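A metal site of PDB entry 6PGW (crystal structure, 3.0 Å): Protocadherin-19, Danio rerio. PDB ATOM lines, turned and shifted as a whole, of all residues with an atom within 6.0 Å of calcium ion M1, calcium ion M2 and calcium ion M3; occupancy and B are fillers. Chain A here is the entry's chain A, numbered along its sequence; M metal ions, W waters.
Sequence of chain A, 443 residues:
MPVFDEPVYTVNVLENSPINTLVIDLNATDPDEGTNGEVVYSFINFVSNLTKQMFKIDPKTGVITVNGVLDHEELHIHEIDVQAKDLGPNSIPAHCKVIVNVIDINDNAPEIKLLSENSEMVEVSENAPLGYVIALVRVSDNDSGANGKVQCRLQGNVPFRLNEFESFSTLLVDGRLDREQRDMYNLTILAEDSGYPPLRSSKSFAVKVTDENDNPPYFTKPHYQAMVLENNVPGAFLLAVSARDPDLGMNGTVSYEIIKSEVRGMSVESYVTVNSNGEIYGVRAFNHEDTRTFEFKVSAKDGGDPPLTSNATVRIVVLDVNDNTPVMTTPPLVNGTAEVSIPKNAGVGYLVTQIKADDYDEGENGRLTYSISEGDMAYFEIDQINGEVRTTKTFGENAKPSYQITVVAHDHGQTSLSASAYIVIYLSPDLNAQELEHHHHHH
The side-chain carboxylate (OD1) of Asp 302 is in hydrogen-bond range of the backbone NH (N) of Leu 308 (2.7 Å). OD2 of Asp 214 sits close to ND2 of Asn 127, 3.3 Å away. The side-chain carboxylate (OE2) of Glu 126 sits close to the backbone NH (N) of Arg 179. OD2 of Asp 211 is in hydrogen-bond range of N of Leu 248 (2.7 Å).
Six residues have an atom within 4 Å of calcium ion M2: Glu 126, Glu 180, Asp 211, Glu 212, Asp 214 and Asp 247.
Of the 22 residues printed, 6 come within 4 Å of calcium ion M3.
Calcium ion M1 is bound by OD2 of Asp 214 (2.3 Å), OE2 of Glu 126 (2.3 Å), OE2 of Glu 180 (2.3 Å), water W1 (2.3 Å), water W2 (2.3 Å) and OD1 of Asp 178 (2.3 Å). Calcium ion M1 has six donor atoms within binding distance.
Calcium ion M2 is bound by the side-chain carboxylate of Glu 126 (2.3 Å), the side-chain carboxylate of Asp 247 (2.3 Å), the side-chain carboxylate of Glu 180 (2.3 Å), the backbone carbonyl oxygen of Glu 212 (2.3 Å), the side-chain carboxylate of Asp 214 (2.3 Å) and the side-chain carboxylate of Asp 211 (2.4 Å). Calcium ion M2 has six donor atoms within binding distance. Slightly farther from calcium ion M2 lies the side-chain carboxylate (OE2) of Glu 180 (3.1 Å).
Calcium ion M3 is bound by the side-chain carboxylate of Asp 302 (2.3 Å), the backbone carbonyl oxygen of Asn 215 (2.3 Å), the backbone carbonyl oxygen of Asn 251 (2.3 Å), the side-chain carboxylate of Asp 245 (2.3 Å), the side-chain carboxylate of Asp 247 (2.3 Å) and the side-chain amide oxygen of Asn 213 (2.3 Å). Calcium ion M3 has six donor atoms within binding distance. Slightly farther from calcium ion M3 lies the side-chain carboxylate (OD1) of Asp 245 (3.0 Å).
Water W1 bridges OD2 of Asp 178 (3.3 Å) and OD1 of Asn 215 (3.5 Å).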
ATOM      1  N   GLU A 126       0.077 -30.146 -22.627  1.00  0.00           N
ATOM      2  CA  GLU A 126       0.978 -30.876 -21.716  1.00  0.00           C
ATOM      3  C   GLU A 126       0.350 -31.138 -20.388  1.00  0.00           C
ATOM      4  O   GLU A 126      -0.360 -30.281 -19.854  1.00  0.00           O
ATOM      5  CB  GLU A 126       2.195 -30.059 -21.364  1.00  0.00           C
ATOM      6  CG  GLU A 126       2.986 -29.482 -22.489  1.00  0.00           C
ATOM      7  CD  GLU A 126       4.183 -28.784 -21.966  1.00  0.00           C
ATOM      8  OE1 GLU A 126       4.173 -27.557 -21.899  1.00  0.00           O
ATOM      9  OE2 GLU A 126       5.080 -29.491 -21.516  1.00  0.00           O
ATOM     10  N   ASN A 127       0.705 -32.265 -19.784  1.00  0.00           N
ATOM     11  CA  ASN A 127       0.204 -32.660 -18.472  1.00  0.00           C
ATOM     12  C   ASN A 127      -1.265 -32.261 -18.279  1.00  0.00           C
ATOM     13  O   ASN A 127      -1.670 -31.802 -17.205  1.00  0.00           O
ATOM     14  CB  ASN A 127       1.116 -32.099 -17.325  1.00  0.00           C
ATOM     15  CG  ASN A 127       1.307 -30.576 -17.380  1.00  0.00           C
ATOM     16  OD1 ASN A 127       0.344 -29.818 -17.482  1.00  0.00           O
ATOM     17  ND2 ASN A 127       2.558 -30.124 -17.312  1.00  0.00           N
ATOM     18  N   LEU A 177       1.858 -36.087 -19.544  1.00  0.00           N
ATOM     19  CA  LEU A 177       2.441 -35.630 -20.802  1.00  0.00           C
ATOM     20  C   LEU A 177       3.347 -34.461 -20.576  1.00  0.00           C
ATOM     21  O   LEU A 177       2.939 -33.445 -20.009  1.00  0.00           O
ATOM     22  CB  LEU A 177       1.363 -35.254 -21.815  1.00  0.00           C
ATOM     23  CG  LEU A 177       0.186 -36.212 -21.950  1.00  0.00           C
ATOM     24  CD1 LEU A 177      -1.040 -35.465 -22.481  1.00  0.00           C
ATOM     25  CD2 LEU A 177       0.565 -37.397 -22.847  1.00  0.00           C
ATOM     26  N   ASP A 178       4.582 -34.589 -21.045  1.00  0.00           N
ATOM     27  CA  ASP A 178       5.549 -33.517 -21.020  1.00  0.00           C
ATOM     28  C   ASP A 178       5.978 -33.244 -22.449  1.00  0.00           C
ATOM     29  O   ASP A 178       6.477 -34.141 -23.124  1.00  0.00           O
ATOM     30  CB  ASP A 178       6.738 -33.926 -20.173  1.00  0.00           C
ATOM     31  CG  ASP A 178       7.631 -32.762 -19.817  1.00  0.00           C
ATOM     32  OD1 ASP A 178       7.332 -31.593 -20.169  1.00  0.00           O
ATOM     33  OD2 ASP A 178       8.655 -33.021 -19.159  1.00  0.00           O
ATOM     34  N   ARG A 179       5.745 -32.006 -22.929  1.00  0.00           N
ATOM     35  CA  ARG A 179       6.147 -31.589 -24.276  1.00  0.00           C
ATOM     36  C   ARG A 179       7.669 -31.555 -24.419  1.00  0.00           C
ATOM     37  O   ARG A 179       8.232 -32.011 -25.429  1.00  0.00           O
ATOM     38  CB  ARG A 179       5.574 -30.208 -24.605  1.00  0.00           C
ATOM     39  CG  ARG A 179       6.178 -29.575 -25.846  1.00  0.00           C
ATOM     40  CD  ARG A 179       5.191 -28.737 -26.600  1.00  0.00           C
ATOM     41  NE  ARG A 179       5.694 -28.421 -27.948  1.00  0.00           N
ATOM     42  CZ  ARG A 179       5.216 -28.934 -29.096  1.00  0.00           C
ATOM     43  NH1 ARG A 179       5.765 -28.553 -30.236  1.00  0.00           N
ATOM     44  NH2 ARG A 179       4.215 -29.828 -29.119  1.00  0.00           N
ATOM     45  N   GLU A 180       8.325 -31.027 -23.383  1.00  0.00           N
ATOM     46  CA  GLU A 180       9.775 -30.945 -23.343  1.00  0.00           C
ATOM     47  C   GLU A 180      10.411 -32.324 -23.538  1.00  0.00           C
ATOM     48  O   GLU A 180      11.518 -32.413 -24.044  1.00  0.00           O
ATOM     49  CB  GLU A 180      10.249 -30.295 -22.039  1.00  0.00           C
ATOM     50  CG  GLU A 180      10.105 -28.762 -22.022  1.00  0.00           C
ATOM     51  CD  GLU A 180       8.651 -28.281 -21.933  1.00  0.00           C
ATOM     52  OE1 GLU A 180       8.303 -27.221 -22.510  1.00  0.00           O
ATOM     53  OE2 GLU A 180       7.850 -28.968 -21.308  1.00  0.00           O
ATOM     54  N   ASP A 211       1.891 -26.925 -26.293  1.00  0.00           N
ATOM     55  CA  ASP A 211       2.811 -26.398 -25.284  1.00  0.00           C
ATOM     56  C   ASP A 211       2.095 -25.580 -24.231  1.00  0.00           C
ATOM     57  O   ASP A 211       1.145 -24.862 -24.512  1.00  0.00           O
ATOM     58  CB  ASP A 211       3.884 -25.523 -25.950  1.00  0.00           C
ATOM     59  CG  ASP A 211       5.015 -25.104 -24.967  1.00  0.00           C
ATOM     60  OD1 ASP A 211       5.547 -25.963 -24.161  1.00  0.00           O
ATOM     61  OD2 ASP A 211       5.357 -23.893 -25.007  1.00  0.00           O
ATOM     62  N   GLU A 212       2.587 -25.708 -23.016  1.00  0.00           N
ATOM     63  CA  GLU A 212       2.227 -24.869 -21.918  1.00  0.00           C
ATOM     64  C   GLU A 212       3.494 -24.179 -21.438  1.00  0.00           C
ATOM     65  O   GLU A 212       4.635 -24.675 -21.673  1.00  0.00           O
ATOM     66  CB  GLU A 212       1.626 -25.713 -20.784  1.00  0.00           C
ATOM     67  CG  GLU A 212       0.131 -25.931 -20.885  1.00  0.00           C
ATOM     68  CD  GLU A 212      -0.641 -24.629 -21.028  1.00  0.00           C
ATOM     69  OE1 GLU A 212      -1.724 -24.652 -21.652  1.00  0.00           O
ATOM     70  OE2 GLU A 212      -0.153 -23.571 -20.544  1.00  0.00           O
ATOM     71  N   ASN A 213       3.295 -23.021 -20.824  1.00  0.00           N
ATOM     72  CA  ASN A 213       4.356 -22.254 -20.231  1.00  0.00           C
ATOM     73  C   ASN A 213       4.505 -22.832 -18.841  1.00  0.00           C
ATOM     74  O   ASN A 213       4.033 -22.271 -17.889  1.00  0.00           O
ATOM     75  CB  ASN A 213       3.911 -20.782 -20.163  1.00  0.00           C
ATOM     76  CG  ASN A 213       5.063 -19.833 -19.888  1.00  0.00           C
ATOM     77  OD1 ASN A 213       6.208 -20.066 -20.275  1.00  0.00           O
ATOM     78  ND2 ASN A 213       4.754 -18.713 -19.223  1.00  0.00           N
ATOM     79  N   ASP A 214       5.061 -24.023 -18.731  1.00  0.00           N
ATOM     80  CA  ASP A 214       5.136 -24.689 -17.427  1.00  0.00           C
ATOM     81  C   ASP A 214       6.513 -24.608 -16.801  1.00  0.00           C
ATOM     82  O   ASP A 214       6.677 -25.003 -15.641  1.00  0.00           O
ATOM     83  CB  ASP A 214       4.597 -26.136 -17.461  1.00  0.00           C
ATOM     84  CG  ASP A 214       5.079 -26.937 -18.650  1.00  0.00           C
ATOM     85  OD1 ASP A 214       5.589 -26.365 -19.663  1.00  0.00           O
ATOM     86  OD2 ASP A 214       4.892 -28.140 -18.560  1.00  0.00           O
ATOM     87  N   ASN A 215       7.487 -24.051 -17.529  1.00  0.00           N
ATOM     88  CA  ASN A 215       8.865 -23.857 -17.033  1.00  0.00           C
ATOM     89  C   ASN A 215       9.287 -22.445 -17.293  1.00  0.00           C
ATOM     90  O   ASN A 215       8.908 -21.899 -18.303  1.00  0.00           O
ATOM     91  CB  ASN A 215       9.813 -24.713 -17.812  1.00  0.00           C
ATOM     92  CG  ASN A 215       9.446 -26.157 -17.779  1.00  0.00           C
ATOM     93  OD1 ASN A 215       9.932 -26.924 -18.584  1.00  0.00           O
ATOM     94  ND2 ASN A 215       8.600 -26.542 -16.839  1.00  0.00           N
ATOM     95  N   PRO A 216      10.143 -21.867 -16.420  1.00  0.00           N
ATOM     96  CA  PRO A 216      10.734 -20.562 -16.693  1.00  0.00           C
ATOM     97  C   PRO A 216      12.143 -20.674 -17.341  1.00  0.00           C
ATOM     98  O   PRO A 216      12.647 -21.807 -17.541  1.00  0.00           O
ATOM     99  CB  PRO A 216      10.844 -19.959 -15.293  1.00  0.00           C
ATOM    100  CG  PRO A 216      11.212 -21.132 -14.448  1.00  0.00           C
ATOM    101  CD  PRO A 216      10.566 -22.354 -15.090  1.00  0.00           C
ATOM    102  N   PRO A 217      12.782 -19.516 -17.634  1.00  0.00           N
ATOM    103  CA  PRO A 217      14.170 -19.547 -18.120  1.00  0.00           C
ATOM    104  C   PRO A 217      15.116 -19.917 -17.000  1.00  0.00           C
ATOM    105  O   PRO A 217      15.131 -19.273 -15.949  1.00  0.00           O
ATOM    106  CB  PRO A 217      14.430 -18.116 -18.617  1.00  0.00           C
ATOM    107  CG  PRO A 217      13.113 -17.414 -18.584  1.00  0.00           C
ATOM    108  CD  PRO A 217      12.264 -18.129 -17.576  1.00  0.00           C
ATOM    109  N   ASP A 245      14.891 -21.086 -21.798  1.00  0.00           N
ATOM    110  CA  ASP A 245      13.584 -21.541 -21.451  1.00  0.00           C
ATOM    111  C   ASP A 245      13.168 -22.621 -22.437  1.00  0.00           C
ATOM    112  O   ASP A 245      13.201 -22.413 -23.661  1.00  0.00           O
ATOM    113  CB  ASP A 245      12.626 -20.385 -21.491  1.00  0.00           C
ATOM    114  CG  ASP A 245      11.264 -20.752 -20.993  1.00  0.00           C
ATOM    115  OD1 ASP A 245      10.680 -21.731 -21.522  1.00  0.00           O
ATOM    116  OD2 ASP A 245      10.757 -20.047 -20.116  1.00  0.00           O
ATOM    117  N   PRO A 246      12.753 -23.779 -21.917  1.00  0.00           N
ATOM    118  CA  PRO A 246      12.463 -24.908 -22.806  1.00  0.00           C
ATOM    119  C   PRO A 246      11.125 -24.857 -23.537  1.00  0.00           C
ATOM    120  O   PRO A 246      10.896 -25.657 -24.412  1.00  0.00           O
ATOM    121  CB  PRO A 246      12.522 -26.115 -21.877  1.00  0.00           C
ATOM    122  CG  PRO A 246      12.219 -25.574 -20.532  1.00  0.00           C
ATOM    123  CD  PRO A 246      12.641 -24.145 -20.501  1.00  0.00           C
ATOM    124  N   ASP A 247      10.256 -23.902 -23.192  1.00  0.00           N
ATOM    125  CA  ASP A 247       8.962 -23.805 -23.840  1.00  0.00           C
ATOM    126  C   ASP A 247       9.009 -23.288 -25.254  1.00  0.00           C
ATOM    127  O   ASP A 247      10.049 -22.838 -25.747  1.00  0.00           O
ATOM    128  CB  ASP A 247       8.067 -22.886 -23.059  1.00  0.00           C
ATOM    129  CG  ASP A 247       7.840 -23.354 -21.712  1.00  0.00           C
ATOM    130  OD1 ASP A 247       7.528 -24.561 -21.566  1.00  0.00           O
ATOM    131  OD2 ASP A 247       8.003 -22.565 -20.785  1.00  0.00           O
ATOM    132  N   LEU A 248       7.845 -23.339 -25.878  1.00  0.00           N
ATOM    133  CA  LEU A 248       7.682 -22.928 -27.253  1.00  0.00           C
ATOM    134  C   LEU A 248       7.415 -21.459 -27.378  1.00  0.00           C
ATOM    135  O   LEU A 248       6.561 -20.902 -26.693  1.00  0.00           O
ATOM    136  CB  LEU A 248       6.559 -23.704 -27.914  1.00  0.00           C
ATOM    137  CG  LEU A 248       7.050 -24.792 -28.840  1.00  0.00           C
ATOM    138  CD1 LEU A 248       7.899 -25.824 -28.105  1.00  0.00           C
ATOM    139  CD2 LEU A 248       5.842 -25.439 -29.529  1.00  0.00           C
ATOM    140  N   MET A 250       6.982 -17.644 -27.357  1.00  0.00           N
ATOM    141  CA  MET A 250       6.852 -16.576 -26.414  1.00  0.00           C
ATOM    142  C   MET A 250       7.030 -17.128 -25.048  1.00  0.00           C
ATOM    143  O   MET A 250       7.577 -16.467 -24.168  1.00  0.00           O
ATOM    144  CB  MET A 250       5.463 -16.056 -26.476  1.00  0.00           C
ATOM    145  CG  MET A 250       5.053 -15.603 -27.856  1.00  0.00           C
ATOM    146  SD  MET A 250       5.021 -13.822 -27.935  1.00  0.00           S
ATOM    147  CE  MET A 250       3.529 -13.459 -26.997  1.00  0.00           C
ATOM    148  N   ASN A 251       6.492 -18.314 -24.827  1.00  0.00           N
ATOM    149  CA  ASN A 251       6.583 -18.938 -23.524  1.00  0.00           C
ATOM    150  C   ASN A 251       8.024 -19.162 -23.152  1.00  0.00           C
ATOM    151  O   ASN A 251       8.387 -19.204 -21.971  1.00  0.00           O
ATOM    152  CB  ASN A 251       5.791 -20.256 -23.486  1.00  0.00           C
ATOM    153  CG  ASN A 251       4.283 -20.056 -23.295  1.00  0.00           C
ATOM    154  OD1 ASN A 251       3.526 -21.019 -23.304  1.00  0.00           O
ATOM    155  ND2 ASN A 251       3.852 -18.808 -23.085  1.00  0.00           N
ATOM    156  N   GLY A 252       8.855 -19.316 -24.181  1.00  0.00           N
ATOM    157  CA  GLY A 252      10.260 -19.620 -24.031  1.00  0.00           C
ATOM    158  C   GLY A 252      11.284 -18.583 -24.506  1.00  0.00           C
ATOM    159  O   GLY A 252      12.467 -18.873 -24.586  1.00  0.00           O
ATOM    160  N   ASP A 302       9.615 -14.367 -19.628  1.00  0.00           N
ATOM    161  CA  ASP A 302       9.173 -14.930 -20.912  1.00  0.00           C
ATOM    162  C   ASP A 302       7.743 -14.559 -21.182  1.00  0.00           C
ATOM    163  O   ASP A 302       6.992 -14.320 -20.251  1.00  0.00           O
ATOM    164  CB  ASP A 302       9.244 -16.435 -20.848  1.00  0.00           C
ATOM    165  CG  ASP A 302       8.440 -16.995 -19.700  1.00  0.00           C
ATOM    166  OD1 ASP A 302       7.981 -16.224 -18.834  1.00  0.00           O
ATOM    167  OD2 ASP A 302       8.277 -18.182 -19.641  1.00  0.00           O
ATOM    168  N   LEU A 308       6.618 -15.868 -16.581  1.00  0.00           N
ATOM    169  CA  LEU A 308       7.386 -16.415 -15.466  1.00  0.00           C
ATOM    170  C   LEU A 308       8.808 -15.852 -15.371  1.00  0.00           C
ATOM    171  O   LEU A 308       9.362 -15.391 -16.363  1.00  0.00           O
ATOM    172  CB  LEU A 308       7.432 -17.933 -15.580  1.00  0.00           C
ATOM    173  CG  LEU A 308       6.058 -18.566 -15.427  1.00  0.00           C
ATOM    174  CD1 LEU A 308       6.190 -20.040 -15.688  1.00  0.00           C
ATOM    175  CD2 LEU A 308       5.464 -18.283 -14.052  1.00  0.00           C
HETATM  176 CA    CA M   1       6.384 -29.524 -19.623  1.00  0.00          CA
HETATM  177 CA    CA M   2       6.179 -26.422 -21.937  1.00  0.00          CA
HETATM  178 CA    CA M   3       8.479 -20.433 -20.023  1.00  0.00          CA
HETATM  179  O   HOH W   1       8.218 -29.914 -18.268  1.00  0.00           O
HETATM  180  O   HOH W   2       5.414 -30.286 -17.650  1.00  0.00           O
